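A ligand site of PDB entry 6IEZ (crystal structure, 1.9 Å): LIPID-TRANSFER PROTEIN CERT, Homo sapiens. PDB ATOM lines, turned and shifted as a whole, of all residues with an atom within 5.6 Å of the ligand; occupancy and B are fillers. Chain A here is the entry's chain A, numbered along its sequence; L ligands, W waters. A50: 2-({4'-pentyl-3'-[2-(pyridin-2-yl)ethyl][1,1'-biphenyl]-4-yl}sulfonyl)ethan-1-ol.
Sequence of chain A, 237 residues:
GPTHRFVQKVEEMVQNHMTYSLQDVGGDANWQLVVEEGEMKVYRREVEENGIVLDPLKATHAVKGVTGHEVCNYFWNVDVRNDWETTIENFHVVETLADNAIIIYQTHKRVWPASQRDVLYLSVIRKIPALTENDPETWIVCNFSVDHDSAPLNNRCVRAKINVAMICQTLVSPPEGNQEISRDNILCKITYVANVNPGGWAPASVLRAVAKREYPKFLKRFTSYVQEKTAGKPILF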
ATOM      1  N   PHE A  75     -27.665  12.760  -7.454  1.00  0.00           N
ATOM      2  CA  PHE A  75     -26.540  12.808  -8.363  1.00  0.00           C
ATOM      3  C   PHE A  75     -25.604  13.944  -7.945  1.00  0.00           C
ATOM      4  O   PHE A  75     -24.385  13.797  -8.005  1.00  0.00           O
ATOM      5  CB  PHE A  75     -27.038  12.862  -9.819  1.00  0.00           C
ATOM      6  CG  PHE A  75     -25.955  12.789 -10.868  1.00  0.00           C
ATOM      7  CD1 PHE A  75     -25.187  11.629 -11.019  1.00  0.00           C
ATOM      8  CD2 PHE A  75     -25.707  13.863 -11.699  1.00  0.00           C
ATOM      9  CE1 PHE A  75     -24.218  11.565 -12.005  1.00  0.00           C
ATOM     10  CE2 PHE A  75     -24.730  13.803 -12.680  1.00  0.00           C
ATOM     11  CZ  PHE A  75     -23.986  12.647 -12.838  1.00  0.00           C
ATOM     12  N   ARG A  81     -22.045  10.690  -2.510  1.00  0.00           N
ATOM     13  CA  ARG A  81     -21.241  10.322  -3.662  1.00  0.00           C
ATOM     14  C   ARG A  81     -20.610   8.942  -3.467  1.00  0.00           C
ATOM     15  O   ARG A  81     -20.759   8.077  -4.329  1.00  0.00           O
ATOM     16  CB  ARG A  81     -20.258  11.449  -3.981  1.00  0.00           C
ATOM     17  CG  ARG A  81     -19.364  11.158  -5.178  1.00  0.00           C
ATOM     18  CD  ARG A  81     -20.113  11.350  -6.499  1.00  0.00           C
ATOM     19  NE  ARG A  81     -20.987  12.502  -6.560  1.00  0.00           N
ATOM     20  CZ  ARG A  81     -20.678  13.680  -7.065  1.00  0.00           C
ATOM     21  NH1 ARG A  81     -21.583  14.649  -7.078  1.00  0.00           N
ATOM     22  NH2 ARG A  81     -19.488  13.907  -7.554  1.00  0.00           N
ATOM     23  N   TRP A  84     -22.571   5.493  -4.139  1.00  0.00           N
ATOM     24  CA  TRP A  84     -22.939   4.922  -5.426  1.00  0.00           C
ATOM     25  C   TRP A  84     -21.751   4.891  -6.411  1.00  0.00           C
ATOM     26  O   TRP A  84     -21.773   4.094  -7.365  1.00  0.00           O
ATOM     27  CB  TRP A  84     -24.194   5.601  -6.013  1.00  0.00           C
ATOM     28  CG  TRP A  84     -24.065   7.075  -6.213  1.00  0.00           C
ATOM     29  CD1 TRP A  84     -24.514   8.053  -5.371  1.00  0.00           C
ATOM     30  CD2 TRP A  84     -23.440   7.759  -7.330  1.00  0.00           C
ATOM     31  NE1 TRP A  84     -24.216   9.300  -5.885  1.00  0.00           N
ATOM     32  CE2 TRP A  84     -23.573   9.155  -7.078  1.00  0.00           C
ATOM     33  CE3 TRP A  84     -22.815   7.345  -8.512  1.00  0.00           C
ATOM     34  CZ2 TRP A  84     -23.078  10.109  -7.961  1.00  0.00           C
ATOM     35  CZ3 TRP A  84     -22.315   8.286  -9.376  1.00  0.00           C
ATOM     36  CH2 TRP A  84     -22.441   9.658  -9.101  1.00  0.00           C
ATOM     37  N   GLU A  85     -20.735   5.735  -6.198  1.00  0.00           N
ATOM     38  CA  GLU A  85     -19.626   5.812  -7.138  1.00  0.00           C
ATOM     39  C   GLU A  85     -18.810   4.539  -6.958  1.00  0.00           C
ATOM     40  O   GLU A  85     -18.616   4.135  -5.808  1.00  0.00           O
ATOM     41  CB  GLU A  85     -18.632   6.930  -6.774  1.00  0.00           C
ATOM     42  CG  GLU A  85     -19.022   8.308  -7.267  1.00  0.00           C
ATOM     43  CD  GLU A  85     -18.637   8.714  -8.679  1.00  0.00           C
ATOM     44  OE1 GLU A  85     -18.482   9.927  -8.900  1.00  0.00           O
ATOM     45  OE2 GLU A  85     -18.508   7.837  -9.575  1.00  0.00           O
ATOM     46  N   THR A  87     -15.900   4.193  -9.367  1.00  0.00           N
ATOM     47  CA  THR A  87     -14.721   4.353 -10.202  1.00  0.00           C
ATOM     48  C   THR A  87     -13.850   5.508  -9.723  1.00  0.00           C
ATOM     49  O   THR A  87     -12.906   5.866 -10.408  1.00  0.00           O
ATOM     50  CB  THR A  87     -15.081   4.522 -11.686  1.00  0.00           C
ATOM     51  OG1 THR A  87     -15.824   5.731 -11.782  1.00  0.00           O
ATOM     52  CG2 THR A  87     -15.878   3.364 -12.247  1.00  0.00           C
ATOM     53  N   ILE A  88     -14.153   6.051  -8.541  1.00  0.00           N
ATOM     54  CA  ILE A  88     -13.509   7.223  -7.976  1.00  0.00           C
ATOM     55  C   ILE A  88     -12.524   6.754  -6.906  1.00  0.00           C
ATOM     56  O   ILE A  88     -12.898   6.061  -5.988  1.00  0.00           O
ATOM     57  CB  ILE A  88     -14.616   8.080  -7.326  1.00  0.00           C
ATOM     58  CG1 ILE A  88     -15.563   8.661  -8.374  1.00  0.00           C
ATOM     59  CG2 ILE A  88     -14.067   9.153  -6.403  1.00  0.00           C
ATOM     60  CD1 ILE A  88     -14.881   9.535  -9.377  1.00  0.00           C
ATOM     61  N   GLN A 106     -11.458  15.266  -8.639  1.00  0.00           N
ATOM     62  CA  GLN A 106     -11.537  13.848  -8.306  1.00  0.00           C
ATOM     63  C   GLN A 106     -10.543  13.067  -9.137  1.00  0.00           C
ATOM     64  O   GLN A 106     -10.135  13.483 -10.222  1.00  0.00           O
ATOM     65  CB  GLN A 106     -12.934  13.249  -8.430  1.00  0.00           C
ATOM     66  CG  GLN A 106     -13.451  13.240  -9.876  1.00  0.00           C
ATOM     67  CD  GLN A 106     -14.940  12.976 -10.007  1.00  0.00           C
ATOM     68  OE1 GLN A 106     -15.772  13.382  -9.169  1.00  0.00           O
ATOM     69  NE2 GLN A 106     -15.316  12.293 -11.085  1.00  0.00           N
ATOM     70  N   HIS A 108      -9.793   9.184 -10.680  1.00  0.00           N
ATOM     71  CA  HIS A 108     -10.432   7.959 -11.089  1.00  0.00           C
ATOM     72  C   HIS A 108      -9.501   6.777 -10.835  1.00  0.00           C
ATOM     73  O   HIS A 108      -8.303   6.898 -11.013  1.00  0.00           O
ATOM     74  CB  HIS A 108     -10.924   8.126 -12.535  1.00  0.00           C
ATOM     75  CG  HIS A 108     -12.206   8.904 -12.542  1.00  0.00           C
ATOM     76  ND1 HIS A 108     -13.424   8.312 -12.317  1.00  0.00           N
ATOM     77  CD2 HIS A 108     -12.441  10.231 -12.617  1.00  0.00           C
ATOM     78  CE1 HIS A 108     -14.377   9.235 -12.308  1.00  0.00           C
ATOM     79  NE2 HIS A 108     -13.794  10.427 -12.493  1.00  0.00           N
ATOM     80  N   VAL A 111      -7.263   2.394 -14.768  1.00  0.00           N
ATOM     81  CA  VAL A 111      -7.625   1.186 -15.503  1.00  0.00           C
ATOM     82  C   VAL A 111      -6.404   0.715 -16.315  1.00  0.00           C
ATOM     83  O   VAL A 111      -6.006   1.343 -17.279  1.00  0.00           O
ATOM     84  CB  VAL A 111      -8.882   1.363 -16.359  1.00  0.00           C
ATOM     85  CG1 VAL A 111      -8.729   2.435 -17.422  1.00  0.00           C
ATOM     86  CG2 VAL A 111      -9.303   0.055 -17.006  1.00  0.00           C
ATOM     87  N   ALA A 114      -3.707   2.097 -18.805  1.00  0.00           N
ATOM     88  CA  ALA A 114      -3.631   3.526 -19.013  1.00  0.00           C
ATOM     89  C   ALA A 114      -3.194   4.204 -17.705  1.00  0.00           C
ATOM     90  O   ALA A 114      -3.349   3.633 -16.622  1.00  0.00           O
ATOM     91  CB  ALA A 114      -4.968   4.015 -19.514  1.00  0.00           C
ATOM     92  N   SER A 115      -2.644   5.419 -17.805  1.00  0.00           N
ATOM     93  CA  SER A 115      -2.355   6.139 -16.571  1.00  0.00           C
ATOM     94  C   SER A 115      -3.642   6.663 -15.939  1.00  0.00           C
ATOM     95  O   SER A 115      -4.694   6.777 -16.568  1.00  0.00           O
ATOM     96  CB  SER A 115      -1.302   7.198 -16.692  1.00  0.00           C
ATOM     97  OG  SER A 115      -1.258   7.748 -17.990  1.00  0.00           O
ATOM     98  N   ARG A 117      -6.429   9.057 -14.462  1.00  0.00           N
ATOM     99  CA  ARG A 117      -6.995  10.342 -14.872  1.00  0.00           C
ATOM    100  C   ARG A 117      -7.531  11.062 -13.637  1.00  0.00           C
ATOM    101  O   ARG A 117      -8.081  10.447 -12.706  1.00  0.00           O
ATOM    102  CB  ARG A 117      -8.137  10.133 -15.887  1.00  0.00           C
ATOM    103  CG  ARG A 117      -7.709  10.297 -17.336  1.00  0.00           C
ATOM    104  CD  ARG A 117      -6.709   9.214 -17.769  1.00  0.00           C
ATOM    105  NE  ARG A 117      -6.310   9.465 -19.140  1.00  0.00           N
ATOM    106  CZ  ARG A 117      -5.293   8.886 -19.746  1.00  0.00           C
ATOM    107  NH1 ARG A 117      -4.604   7.927 -19.144  1.00  0.00           N
ATOM    108  NH2 ARG A 117      -4.926   9.309 -20.942  1.00  0.00           N
ATOM    109  N   VAL A 119      -9.937  14.865 -12.782  1.00  0.00           N
ATOM    110  CA  VAL A 119     -10.900  15.741 -13.406  1.00  0.00           C
ATOM    111  C   VAL A 119     -11.103  16.928 -12.471  1.00  0.00           C
ATOM    112  O   VAL A 119     -11.039  16.760 -11.250  1.00  0.00           O
ATOM    113  CB  VAL A 119     -12.248  15.029 -13.638  1.00  0.00           C
ATOM    114  CG1 VAL A 119     -13.112  15.764 -14.660  1.00  0.00           C
ATOM    115  CG2 VAL A 119     -12.054  13.565 -14.060  1.00  0.00           C
ATOM    116  N   TYR A 121     -14.010  19.969 -12.197  1.00  0.00           N
ATOM    117  CA  TYR A 121     -15.230  20.342 -12.880  1.00  0.00           C
ATOM    118  C   TYR A 121     -16.185  21.084 -11.932  1.00  0.00           C
ATOM    119  O   TYR A 121     -16.268  20.791 -10.740  1.00  0.00           O
ATOM    120  CB  TYR A 121     -15.920  19.095 -13.480  1.00  0.00           C
ATOM    121  CG  TYR A 121     -16.379  18.085 -12.467  1.00  0.00           C
ATOM    122  CD1 TYR A 121     -15.520  17.089 -12.007  1.00  0.00           C
ATOM    123  CD2 TYR A 121     -17.698  18.052 -12.027  1.00  0.00           C
ATOM    124  CE1 TYR A 121     -15.939  16.135 -11.102  1.00  0.00           C
ATOM    125  CE2 TYR A 121     -18.130  17.101 -11.107  1.00  0.00           C
ATOM    126  CZ  TYR A 121     -17.240  16.131 -10.653  1.00  0.00           C
ATOM    127  OH  TYR A 121     -17.616  15.188  -9.741  1.00  0.00           O
ATOM    128  N   ASN A 143     -22.194  18.701 -15.120  1.00  0.00           N
ATOM    129  CA  ASN A 143     -20.828  18.652 -14.641  1.00  0.00           C
ATOM    130  C   ASN A 143     -19.913  18.967 -15.806  1.00  0.00           C
ATOM    131  O   ASN A 143     -19.820  18.160 -16.731  1.00  0.00           O
ATOM    132  CB  ASN A 143     -20.505  17.247 -14.092  1.00  0.00           C
ATOM    133  CG  ASN A 143     -21.315  16.934 -12.856  1.00  0.00           C
ATOM    134  OD1 ASN A 143     -21.669  17.840 -12.120  1.00  0.00           O
ATOM    135  ND2 ASN A 143     -21.624  15.668 -12.606  1.00  0.00           N
ATOM    136  N   ALA A 160      -8.378  14.693 -17.378  1.00  0.00           N
ATOM    137  CA  ALA A 160      -9.424  14.498 -18.371  1.00  0.00           C
ATOM    138  C   ALA A 160     -10.328  15.731 -18.367  1.00  0.00           C
ATOM    139  O   ALA A 160     -10.366  16.446 -17.368  1.00  0.00           O
ATOM    140  CB  ALA A 160     -10.238  13.308 -17.956  1.00  0.00           C
ATOM    141  N   ILE A 162     -14.449  16.965 -19.111  1.00  0.00           N
ATOM    142  CA  ILE A 162     -15.755  16.360 -19.213  1.00  0.00           C
ATOM    143  C   ILE A 162     -16.794  17.440 -19.418  1.00  0.00           C
ATOM    144  O   ILE A 162     -16.636  18.594 -19.004  1.00  0.00           O
ATOM    145  CB  ILE A 162     -16.083  15.509 -17.969  1.00  0.00           C
ATOM    146  CG1 ILE A 162     -16.442  16.372 -16.762  1.00  0.00           C
ATOM    147  CG2 ILE A 162     -14.957  14.531 -17.674  1.00  0.00           C
ATOM    148  CD1 ILE A 162     -16.987  15.594 -15.589  1.00  0.00           C
ATOM    149  N   VAL A 164     -20.839  16.577 -18.800  1.00  0.00           N
ATOM    150  CA  VAL A 164     -21.773  15.527 -18.469  1.00  0.00           C
ATOM    151  C   VAL A 164     -23.060  16.242 -18.066  1.00  0.00           C
ATOM    152  O   VAL A 164     -22.989  17.289 -17.444  1.00  0.00           O
ATOM    153  CB  VAL A 164     -21.219  14.681 -17.311  1.00  0.00           C
ATOM    154  CG1 VAL A 164     -22.305  13.822 -16.685  1.00  0.00           C
ATOM    155  CG2 VAL A 164     -20.023  13.828 -17.722  1.00  0.00           C
ATOM    156  N   TYR A 192     -29.014  10.950 -20.016  1.00  0.00           N
ATOM    157  CA  TYR A 192     -27.680  11.169 -19.458  1.00  0.00           C
ATOM    158  C   TYR A 192     -26.686  11.284 -20.626  1.00  0.00           C
ATOM    159  O   TYR A 192     -26.631  10.404 -21.490  1.00  0.00           O
ATOM    160  CB  TYR A 192     -27.318  10.008 -18.510  1.00  0.00           C
ATOM    161  CG  TYR A 192     -25.871  10.005 -18.065  1.00  0.00           C
ATOM    162  CD1 TYR A 192     -25.469  10.709 -16.944  1.00  0.00           C
ATOM    163  CD2 TYR A 192     -24.886   9.340 -18.809  1.00  0.00           C
ATOM    164  CE1 TYR A 192     -24.138  10.727 -16.531  1.00  0.00           C
ATOM    165  CE2 TYR A 192     -23.561   9.371 -18.415  1.00  0.00           C
ATOM    166  CZ  TYR A 192     -23.186  10.044 -17.273  1.00  0.00           C
ATOM    167  OH  TYR A 192     -21.869  10.080 -16.926  1.00  0.00           O
ATOM    168  N   VAL A 196     -16.372  13.042 -22.794  1.00  0.00           N
ATOM    169  CA  VAL A 196     -15.150  12.972 -22.011  1.00  0.00           C
ATOM    170  C   VAL A 196     -13.963  12.972 -22.939  1.00  0.00           C
ATOM    171  O   VAL A 196     -13.880  12.144 -23.856  1.00  0.00           O
ATOM    172  CB  VAL A 196     -15.162  11.697 -21.147  1.00  0.00           C
ATOM    173  CG1 VAL A 196     -13.821  11.545 -20.423  1.00  0.00           C
ATOM    174  CG2 VAL A 196     -16.338  11.751 -20.195  1.00  0.00           C
ATOM    175  N   PRO A 198     -10.250  12.103 -22.526  1.00  0.00           N
ATOM    176  CA  PRO A 198      -9.384  11.494 -21.513  1.00  0.00           C
ATOM    177  C   PRO A 198      -8.003  12.154 -21.387  1.00  0.00           C
ATOM    178  O   PRO A 198      -7.241  11.883 -20.456  1.00  0.00           O
ATOM    179  CB  PRO A 198      -9.256  10.030 -21.989  1.00  0.00           C
ATOM    180  CG  PRO A 198      -9.443  10.131 -23.490  1.00  0.00           C
ATOM    181  CD  PRO A 198     -10.513  11.205 -23.667  1.00  0.00           C
ATOM    182  N   ALA A 202      -4.498   7.115 -24.418  1.00  0.00           N
ATOM    183  CA  ALA A 202      -4.830   5.867 -23.763  1.00  0.00           C
ATOM    184  C   ALA A 202      -5.227   4.916 -24.884  1.00  0.00           C
ATOM    185  O   ALA A 202      -5.696   5.417 -25.909  1.00  0.00           O
ATOM    186  CB  ALA A 202      -5.963   6.055 -22.789  1.00  0.00           C
ATOM    187  N   VAL A 206      -9.055   0.141 -24.716  1.00  0.00           N
ATOM    188  CA  VAL A 206      -9.284   0.290 -23.283  1.00  0.00           C
ATOM    189  C   VAL A 206     -10.423   1.285 -23.022  1.00  0.00           C
ATOM    190  O   VAL A 206     -11.411   0.938 -22.375  1.00  0.00           O
ATOM    191  CB  VAL A 206      -7.994   0.656 -22.554  1.00  0.00           C
ATOM    192  CG1 VAL A 206      -8.232   0.846 -21.060  1.00  0.00           C
ATOM    193  CG2 VAL A 206      -6.900  -0.382 -22.817  1.00  0.00           C
ATOM    194  N   LEU A 207     -10.287   2.517 -23.520  1.00  0.00           N
ATOM    195  CA  LEU A 207     -11.310   3.535 -23.417  1.00  0.00           C
ATOM    196  C   LEU A 207     -12.686   2.964 -23.788  1.00  0.00           C
ATOM    197  O   LEU A 207     -13.661   3.157 -23.076  1.00  0.00           O
ATOM    198  CB  LEU A 207     -10.931   4.714 -24.332  1.00  0.00           C
ATOM    199  CG  LEU A 207      -9.707   5.483 -23.835  1.00  0.00           C
ATOM    200  CD1 LEU A 207      -9.252   6.554 -24.825  1.00  0.00           C
ATOM    201  CD2 LEU A 207     -10.006   6.096 -22.481  1.00  0.00           C
ATOM    202  N   VAL A 210     -13.901   0.343 -21.212  1.00  0.00           N
ATOM    203  CA  VAL A 210     -14.266   0.929 -19.932  1.00  0.00           C
ATOM    204  C   VAL A 210     -15.653   1.574 -20.075  1.00  0.00           C
ATOM    205  O   VAL A 210     -16.509   1.398 -19.225  1.00  0.00           O
ATOM    206  CB  VAL A 210     -13.228   1.962 -19.465  1.00  0.00           C
ATOM    207  CG1 VAL A 210     -13.712   2.700 -18.206  1.00  0.00           C
ATOM    208  CG2 VAL A 210     -11.868   1.311 -19.227  1.00  0.00           C
ATOM    209  N   ALA A 211     -15.851   2.332 -21.165  1.00  0.00           N
ATOM    210  CA  ALA A 211     -17.121   3.018 -21.351  1.00  0.00           C
ATOM    211  C   ALA A 211     -18.265   1.998 -21.439  1.00  0.00           C
ATOM    212  O   ALA A 211     -19.336   2.172 -20.853  1.00  0.00           O
ATOM    213  CB  ALA A 211     -17.059   3.858 -22.598  1.00  0.00           C
ATOM    214  N   GLU A 214     -18.670   0.478 -17.881  1.00  0.00           N
ATOM    215  CA  GLU A 214     -18.916   1.320 -16.708  1.00  0.00           C
ATOM    216  C   GLU A 214     -20.152   2.193 -16.839  1.00  0.00           C
ATOM    217  O   GLU A 214     -20.796   2.436 -15.833  1.00  0.00           O
ATOM    218  CB  GLU A 214     -17.682   2.138 -16.291  1.00  0.00           C
ATOM    219  CG  GLU A 214     -16.461   1.312 -15.858  1.00  0.00           C
ATOM    220  CD  GLU A 214     -16.670   0.349 -14.693  1.00  0.00           C
ATOM    221  OE1 GLU A 214     -17.604   0.577 -13.877  1.00  0.00           O
ATOM    222  OE2 GLU A 214     -15.923  -0.661 -14.617  1.00  0.00           O
ATOM    223  N   TYR A 215     -20.528   2.651 -18.040  1.00  0.00           N
ATOM    224  CA  TYR A 215     -21.719   3.504 -18.130  1.00  0.00           C
ATOM    225  C   TYR A 215     -23.008   2.767 -17.753  1.00  0.00           C
ATOM    226  O   TYR A 215     -23.771   3.265 -16.904  1.00  0.00           O
ATOM    227  CB  TYR A 215     -21.813   4.292 -19.440  1.00  0.00           C
ATOM    228  CG  TYR A 215     -20.852   5.470 -19.541  1.00  0.00           C
ATOM    229  CD1 TYR A 215     -20.913   6.556 -18.668  1.00  0.00           C
ATOM    230  CD2 TYR A 215     -19.860   5.485 -20.498  1.00  0.00           C
ATOM    231  CE1 TYR A 215     -20.040   7.639 -18.770  1.00  0.00           C
ATOM    232  CE2 TYR A 215     -18.989   6.550 -20.623  1.00  0.00           C
ATOM    233  CZ  TYR A 215     -19.074   7.635 -19.770  1.00  0.00           C
ATOM    234  OH  TYR A 215     -18.171   8.650 -19.964  1.00  0.00           O
ATOM    235  N   PHE A 218     -22.915   2.068 -14.068  1.00  0.00           N
ATOM    236  CA  PHE A 218     -23.150   3.286 -13.307  1.00  0.00           C
ATOM    237  C   PHE A 218     -24.656   3.592 -13.275  1.00  0.00           C
ATOM    238  O   PHE A 218     -25.207   3.811 -12.203  1.00  0.00           O
ATOM    239  CB  PHE A 218     -22.304   4.460 -13.849  1.00  0.00           C
ATOM    240  CG  PHE A 218     -23.014   5.781 -13.732  1.00  0.00           C
ATOM    241  CD1 PHE A 218     -23.255   6.329 -12.476  1.00  0.00           C
ATOM    242  CD2 PHE A 218     -23.507   6.436 -14.858  1.00  0.00           C
ATOM    243  CE1 PHE A 218     -23.948   7.534 -12.364  1.00  0.00           C
ATOM    244  CE2 PHE A 218     -24.205   7.632 -14.735  1.00  0.00           C
ATOM    245  CZ  PHE A 218     -24.404   8.186 -13.485  1.00  0.00           C
HETATM  246  C12 A50 L   1     -17.522  12.213 -14.385  1.00  0.00           C
HETATM  247  C13 A50 L   1     -14.213   7.684 -19.194  1.00  0.00           C
HETATM  248  C14 A50 L   1     -14.126   6.227 -18.631  1.00  0.00           C
HETATM  249  C15 A50 L   1     -17.284   5.574 -15.856  1.00  0.00           C
HETATM  250  C17 A50 L   1     -16.584   5.843 -18.154  1.00  0.00           C
HETATM  251  C18 A50 L   1     -15.251   5.968 -17.682  1.00  0.00           C
HETATM  252  C19 A50 L   1     -15.948   5.721 -15.476  1.00  0.00           C
HETATM  253  C20 A50 L   1     -20.389  11.544 -12.008  1.00  0.00           C
HETATM  254  N1  A50 L   1     -14.928   5.930 -16.356  1.00  0.00           N
HETATM  255  C5  A50 L   1     -15.224   9.115 -17.373  1.00  0.00           C
HETATM  256  C6  A50 L   1     -15.103  10.053 -16.315  1.00  0.00           C
HETATM  257  C7  A50 L   1     -18.655  11.423 -14.468  1.00  0.00           C
HETATM  258  C9  A50 L   1     -17.508   9.768 -15.737  1.00  0.00           C
HETATM  259  O2  A50 L   1     -20.046  13.502 -13.888  1.00  0.00           O
HETATM  260  S1  A50 L   1     -20.175  12.043 -13.769  1.00  0.00           S
HETATM  261  O1  A50 L   1     -21.262  11.314 -14.447  1.00  0.00           O
HETATM  262  C21 A50 L   1     -19.241  12.190 -11.200  1.00  0.00           C
HETATM  263  O3  A50 L   1     -18.112  11.330 -11.184  1.00  0.00           O
HETATM  264  C11 A50 L   1     -16.334  11.753 -14.992  1.00  0.00           C
HETATM  265  C10 A50 L   1     -16.328  10.522 -15.661  1.00  0.00           C
HETATM  266  C8  A50 L   1     -18.719  10.192 -15.129  1.00  0.00           C
HETATM  267  C1  A50 L   1     -13.823  10.576 -15.999  1.00  0.00           C
HETATM  268  C23 A50 L   1     -12.654  10.162 -16.681  1.00  0.00           C
HETATM  269  C3  A50 L   1     -12.791   9.205 -17.723  1.00  0.00           C
HETATM  270  C24 A50 L   1     -11.567   8.772 -18.488  1.00  0.00           C
HETATM  271  C25 A50 L   1     -10.925   7.575 -17.802  1.00  0.00           C
HETATM  272  C26 A50 L   1      -9.719   7.179 -18.639  1.00  0.00           C
HETATM  273  C27 A50 L   1      -9.464   5.704 -18.352  1.00  0.00           C
HETATM  274  C28 A50 L   1      -8.148   5.331 -19.029  1.00  0.00           C
HETATM  275  C4  A50 L   1     -14.070   8.694 -18.067  1.00  0.00           C
HETATM  276  C16 A50 L   1     -17.624   5.626 -17.224  1.00  0.00           C
HETATM  277  O   HOH W   1     -18.099   8.696 -11.868  1.00  0.00           O
HETATM  278  O   HOH W   2      -6.802   4.652 -16.157  1.00  0.00           O
HETATM  279  O   HOH W   3     -12.346   6.045 -14.755  1.00  0.00           O
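CZ of Phe 75 touches O1 of the ligand, 3.4 Å away. Thr 87 touches the ligand. His 108 touches the ligand. Val 111 touches the ligand (CG1 to C28, 3.4 Å). CB of Ala 114 touches C28 of the ligand, 3.5 Å away. Arg 117 touches the ligand. Val 119 touches the ligand (CG2 to C1, 3.98 Å). Tyr 121 touches the ligand (OH to C21, 3.7 Å). CD1 of Ile 162 touches C12 of the ligand, at 3.6 Å. Val 164 touches the ligand (CG1 to O1, 3.5 Å). Val 196 touches the ligand (CG1 to C4, 3.7 Å). Leu 207 touches the ligand. Val 210 touches the ligand (CG1 to C14, 3.6 Å). Glu 214 touches the ligand. CZ of Tyr 215 touches C17 of the ligand, at 3.5 Å. Hydrophobic or aromatic side chains within 4 Å of the ligand: Phe 75, His 108, Val 111, Ala 114, Val 119, Ile 162, Val 164, Tyr 192, Val 196, Leu 207, Val 210 and Tyr 215. Within 4 Å of the ligand: Phe 75, Glu 85, Thr 87, Gln 106, His 108, Val 111, Ala 114, Arg 117, Val 119, Tyr 121, Asn 143, Ile 162, Val 164, Tyr 192, Val 196, Leu 207, Val 210, Glu 214 and Tyr 215.
OE1 of Glu 85 is in hydrogen-bond range of O3 of the ligand. An oxygen (O1) of the ligand is in hydrogen-bond range of the side-chain hydroxyl (OH) of Tyr 192 (2.8 Å). NE2 of Gln 106 lies within hydrogen-bond range of O3 of the ligand, at 3.0 Å. ND2 of Asn 143 sits at hydrogen-bond distance from O2 of the ligand (3.0 Å).
Water W1 lies within hydrogen-bond range of the side-chain carboxylate (OE2) of Glu 85 (2.5 Å) and an oxygen (O3) of the ligand (2.7 Å). Water W3 bridges a nitrogen (N1) of the ligand (3.0 Å) and a ring nitrogen (ND1) of His 108 (3.5 Å).
The side-chain hydroxyl (OH) of Tyr 121 sits at hydrogen-bond distance from the side-chain amide oxygen (OE1) of Gln 106 (2.6 Å). The backbone NH (N) of Val 119 lies within hydrogen-bond range of the backbone carbonyl oxygen (O) of Gln 106 (2.9 Å). The backbone carbonyl oxygen (O) of Phe 75 is in hydrogen-bond range of the guanidinium group (NH1) of Arg 81, at 3.1 Å. A ring nitrogen (ND1) of His 108 lies within hydrogen-bond range of the backbone carbonyl oxygen (O) of Thr 87 (3.1 Å). The backbone carbonyl oxygen (O) of Arg 117 sits at hydrogen-bond distance from the backbone NH (N) of His 108, 2.9 Å away. NH2 of Arg 81 is in hydrogen-bond range of OH of Tyr 121. The backbone carbonyl oxygen of Pro 198 sits at hydrogen-bond distance from the guanidinium group of Arg 117. The guanidinium group (NH1) of Arg 117 lies within hydrogen-bond range of the backbone carbonyl oxygen (O) of Ser 115.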
